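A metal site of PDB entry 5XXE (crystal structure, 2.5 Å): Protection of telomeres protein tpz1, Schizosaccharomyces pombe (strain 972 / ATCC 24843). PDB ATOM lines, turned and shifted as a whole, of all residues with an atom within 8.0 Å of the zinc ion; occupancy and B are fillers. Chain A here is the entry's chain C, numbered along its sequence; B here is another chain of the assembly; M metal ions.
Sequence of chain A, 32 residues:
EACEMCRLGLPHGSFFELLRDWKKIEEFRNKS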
ATOM      1  N   GLU A   1      29.307 -13.261 -23.090  1.00  0.00           N
ATOM      2  CA  GLU A   1      28.253 -13.522 -24.126  1.00  0.00           C
ATOM      3  C   GLU A   1      26.846 -13.566 -23.525  1.00  0.00           C
ATOM      4  O   GLU A   1      25.925 -12.959 -24.058  1.00  0.00           O
ATOM      5  CB  GLU A   1      28.532 -14.821 -24.888  1.00  0.00           C
ATOM      6  CG  GLU A   1      29.834 -14.801 -25.685  1.00  0.00           C
ATOM      7  CD  GLU A   1      29.844 -15.732 -26.892  1.00  0.00           C
ATOM      8  OE1 GLU A   1      28.802 -15.881 -27.572  1.00  0.00           O
ATOM      9  OE2 GLU A   1      30.916 -16.310 -27.180  1.00  0.00           O
ATOM     10  N   ALA A   2      26.693 -14.292 -22.411  1.00  0.00           N
ATOM     11  CA  ALA A   2      25.401 -14.357 -21.705  1.00  0.00           C
ATOM     12  C   ALA A   2      25.028 -13.016 -21.082  1.00  0.00           C
ATOM     13  O   ALA A   2      23.920 -12.507 -21.293  1.00  0.00           O
ATOM     14  CB  ALA A   2      25.433 -15.434 -20.645  1.00  0.00           C
ATOM     15  N   CYS A   3      25.954 -12.443 -20.315  1.00  0.00           N
ATOM     16  CA  CYS A   3      25.754 -11.124 -19.710  1.00  0.00           C
ATOM     17  C   CYS A   3      25.837 -10.024 -20.763  1.00  0.00           C
ATOM     18  O   CYS A   3      26.902  -9.747 -21.298  1.00  0.00           O
ATOM     19  CB  CYS A   3      26.793 -10.859 -18.616  1.00  0.00           C
ATOM     20  SG  CYS A   3      26.665  -9.201 -17.930  1.00  0.00           S
ATOM     21  N   GLU A   4      24.714  -9.372 -21.020  1.00  0.00           N
ATOM     22  CA  GLU A   4      24.644  -8.399 -22.119  1.00  0.00           C
ATOM     23  C   GLU A   4      25.344  -7.084 -21.765  1.00  0.00           C
ATOM     24  O   GLU A   4      25.720  -6.336 -22.672  1.00  0.00           O
ATOM     25  CB  GLU A   4      23.207  -8.160 -22.645  1.00  0.00           C
ATOM     26  CG  GLU A   4      22.029  -8.302 -21.669  1.00  0.00           C
ATOM     27  CD  GLU A   4      21.586  -9.752 -21.444  1.00  0.00           C
ATOM     28  OE1 GLU A   4      21.192 -10.422 -22.420  1.00  0.00           O
ATOM     29  OE2 GLU A   4      21.630 -10.210 -20.285  1.00  0.00           O
ATOM     30  N   MET A   5      25.553  -6.818 -20.473  1.00  0.00           N
ATOM     31  CA  MET A   5      26.381  -5.687 -20.046  1.00  0.00           C
ATOM     32  C   MET A   5      27.824  -5.942 -20.390  1.00  0.00           C
ATOM     33  O   MET A   5      28.496  -5.034 -20.873  1.00  0.00           O
ATOM     34  CB  MET A   5      26.258  -5.366 -18.553  1.00  0.00           C
ATOM     35  CG  MET A   5      24.878  -4.843 -18.169  1.00  0.00           C
ATOM     36  SD  MET A   5      24.483  -3.127 -19.071  1.00  0.00           S
ATOM     37  CE  MET A   5      25.405  -1.946 -17.779  1.00  0.00           C
ATOM     38  N   CYS A   6      28.321  -7.163 -20.154  1.00  0.00           N
ATOM     39  CA  CYS A   6      29.664  -7.560 -20.592  1.00  0.00           C
ATOM     40  C   CYS A   6      29.840  -7.392 -22.108  1.00  0.00           C
ATOM     41  O   CYS A   6      30.773  -6.723 -22.538  1.00  0.00           O
ATOM     42  CB  CYS A   6      30.007  -9.007 -20.186  1.00  0.00           C
ATOM     43  SG  CYS A   6      30.343  -9.289 -18.424  1.00  0.00           S
ATOM     44  N   ARG A   7      28.930  -7.966 -22.907  1.00  0.00           N
ATOM     45  CA  ARG A   7      28.930  -7.770 -24.372  1.00  0.00           C
ATOM     46  C   ARG A   7      29.004  -6.313 -24.794  1.00  0.00           C
ATOM     47  O   ARG A   7      29.751  -5.960 -25.691  1.00  0.00           O
ATOM     48  CB  ARG A   7      27.687  -8.407 -25.025  1.00  0.00           C
ATOM     49  CG  ARG A   7      27.903  -9.836 -25.480  1.00  0.00           C
ATOM     50  CD  ARG A   7      26.654 -10.442 -26.106  1.00  0.00           C
ATOM     51  NE  ARG A   7      26.554 -10.233 -27.547  1.00  0.00           N
ATOM     52  CZ  ARG A   7      25.602 -10.748 -28.326  1.00  0.00           C
ATOM     53  NH1 ARG A   7      24.623 -11.498 -27.813  1.00  0.00           N
ATOM     54  NH2 ARG A   7      25.615 -10.503 -29.630  1.00  0.00           N
ATOM     55  N   LEU A   8      28.210  -5.473 -24.139  1.00  0.00           N
ATOM     56  CA  LEU A   8      28.198  -4.021 -24.405  1.00  0.00           C
ATOM     57  C   LEU A   8      29.446  -3.270 -23.899  1.00  0.00           C
ATOM     58  O   LEU A   8      29.618  -2.101 -24.232  1.00  0.00           O
ATOM     59  CB  LEU A   8      26.938  -3.389 -23.794  1.00  0.00           C
ATOM     60  CG  LEU A   8      25.607  -3.724 -24.479  1.00  0.00           C
ATOM     61  CD1 LEU A   8      24.419  -3.528 -23.537  1.00  0.00           C
ATOM     62  CD2 LEU A   8      25.443  -2.894 -25.732  1.00  0.00           C
ATOM     63  N   LEU A  10      29.964  -2.173 -20.905  1.00  0.00           N
ATOM     64  CA  LEU A  10      29.517  -1.157 -19.949  1.00  0.00           C
ATOM     65  C   LEU A  10      29.808  -1.610 -18.524  1.00  0.00           C
ATOM     66  O   LEU A  10      29.832  -2.820 -18.265  1.00  0.00           O
ATOM     67  CB  LEU A  10      28.011  -0.913 -20.091  1.00  0.00           C
ATOM     68  CG  LEU A  10      27.542  -0.371 -21.432  1.00  0.00           C
ATOM     69  CD1 LEU A  10      26.021  -0.411 -21.510  1.00  0.00           C
ATOM     70  CD2 LEU A  10      28.071   1.042 -21.666  1.00  0.00           C
ATOM     71  N   PRO A  11      30.031  -0.659 -17.603  1.00  0.00           N
ATOM     72  CA  PRO A  11      30.376  -1.033 -16.232  1.00  0.00           C
ATOM     73  C   PRO A  11      29.156  -1.479 -15.404  1.00  0.00           C
ATOM     74  O   PRO A  11      28.063  -0.899 -15.522  1.00  0.00           O
ATOM     75  CB  PRO A  11      30.991   0.243 -15.672  1.00  0.00           C
ATOM     76  CG  PRO A  11      30.294   1.344 -16.395  1.00  0.00           C
ATOM     77  CD  PRO A  11      29.898   0.807 -17.752  1.00  0.00           C
ATOM     78  N   HIS A  12      29.374  -2.483 -14.557  1.00  0.00           N
ATOM     79  CA  HIS A  12      28.310  -3.100 -13.758  1.00  0.00           C
ATOM     80  C   HIS A  12      28.929  -4.065 -12.737  1.00  0.00           C
ATOM     81  O   HIS A  12      30.071  -4.500 -12.915  1.00  0.00           O
ATOM     82  CB  HIS A  12      27.337  -3.863 -14.656  1.00  0.00           C
ATOM     83  CG  HIS A  12      27.968  -4.979 -15.429  1.00  0.00           C
ATOM     84  ND1 HIS A  12      28.918  -4.766 -16.414  1.00  0.00           N
ATOM     85  CD2 HIS A  12      27.789  -6.317 -15.371  1.00  0.00           C
ATOM     86  CE1 HIS A  12      29.291  -5.933 -16.910  1.00  0.00           C
ATOM     87  NE2 HIS A  12      28.616  -6.892 -16.301  1.00  0.00           N
ATOM     88  N   GLY A  13      28.162  -4.399 -11.694  1.00  0.00           N
ATOM     89  CA  GLY A  13      28.597  -5.354 -10.661  1.00  0.00           C
ATOM     90  C   GLY A  13      28.844  -4.666  -9.347  1.00  0.00           C
ATOM     91  O   GLY A  13      28.687  -3.468  -9.241  1.00  0.00           O
ATOM     92  N   LYS B  46      36.656  -4.891 -16.332  1.00  0.00           N
ATOM     93  CA  LYS B  46      35.851  -5.947 -16.961  1.00  0.00           C
ATOM     94  C   LYS B  46      35.915  -7.280 -16.227  1.00  0.00           C
ATOM     95  O   LYS B  46      34.906  -7.953 -16.088  1.00  0.00           O
ATOM     96  CB  LYS B  46      36.262  -6.132 -18.425  1.00  0.00           C
ATOM     97  CG  LYS B  46      35.848  -4.960 -19.304  1.00  0.00           C
ATOM     98  CD  LYS B  46      36.409  -5.079 -20.718  1.00  0.00           C
ATOM     99  CE  LYS B  46      35.783  -4.041 -21.642  1.00  0.00           C
ATOM    100  NZ  LYS B  46      35.918  -2.641 -21.132  1.00  0.00           N
ATOM    101  N   MET B  48      36.271  -7.834 -13.028  1.00  0.00           N
ATOM    102  CA  MET B  48      35.726  -7.788 -11.658  1.00  0.00           C
ATOM    103  C   MET B  48      34.207  -7.689 -11.582  1.00  0.00           C
ATOM    104  O   MET B  48      33.648  -7.628 -10.482  1.00  0.00           O
ATOM    105  CB  MET B  48      36.349  -6.587 -10.937  1.00  0.00           C
ATOM    106  CG  MET B  48      37.867  -6.703 -10.783  1.00  0.00           C
ATOM    107  SD  MET B  48      38.408  -8.000  -9.400  1.00  0.00           S
ATOM    108  CE  MET B  48      39.352  -9.277 -10.571  1.00  0.00           C
ATOM    109  N   CYS B  49      33.530  -7.711 -12.727  1.00  0.00           N
ATOM    110  CA  CYS B  49      32.093  -7.461 -12.800  1.00  0.00           C
ATOM    111  C   CYS B  49      31.230  -8.515 -12.103  1.00  0.00           C
ATOM    112  O   CYS B  49      30.168  -8.196 -11.557  1.00  0.00           O
ATOM    113  CB  CYS B  49      31.655  -7.348 -14.264  1.00  0.00           C
ATOM    114  SG  CYS B  49      32.202  -5.824 -15.074  1.00  0.00           S
ATOM    115  N   HIS B  50      31.676  -9.777 -12.134  1.00  0.00           N
ATOM    116  CA  HIS B  50      30.929 -10.885 -11.540  1.00  0.00           C
ATOM    117  C   HIS B  50      31.794 -11.607 -10.518  1.00  0.00           C
ATOM    118  O   HIS B  50      31.760 -12.835 -10.405  1.00  0.00           O
ATOM    119  CB  HIS B  50      30.488 -11.847 -12.649  1.00  0.00           C
ATOM    120  CG  HIS B  50      29.722 -11.174 -13.758  1.00  0.00           C
ATOM    121  ND1 HIS B  50      28.406 -10.804 -13.625  1.00  0.00           N
ATOM    122  CD2 HIS B  50      30.094 -10.808 -15.000  1.00  0.00           C
ATOM    123  CE1 HIS B  50      27.992 -10.234 -14.739  1.00  0.00           C
ATOM    124  NE2 HIS B  50      29.004 -10.213 -15.589  1.00  0.00           N
HETATM  125 ZN    ZN M   1      28.700  -8.855 -16.942  1.00  0.00          ZN
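The backbone carbonyl oxygen of His 12 lies within hydrogen-bond range of the side-chain sulfur of Cys 49 of chain B (3.3 Å).
A ring nitrogen (ND1) of His 12 lies within hydrogen-bond range of the backbone carbonyl oxygen (O) of Leu 10 (2.8 Å).
The backbone NH (N) of Met 5 sits close to the side-chain sulfur (SG) of Cys 3.
The zinc ion is bound by NE2 of His 50 of chain B (1.9 Å).
The zinc ion is bound by a ring nitrogen (NE2) of His 12 (2.1 Å).
SG of Cys 6 binds the zinc ion, 2.3 Å away.
The zinc ion is bound by the side-chain sulfur (SG) of Cys 3 (2.3 Å).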
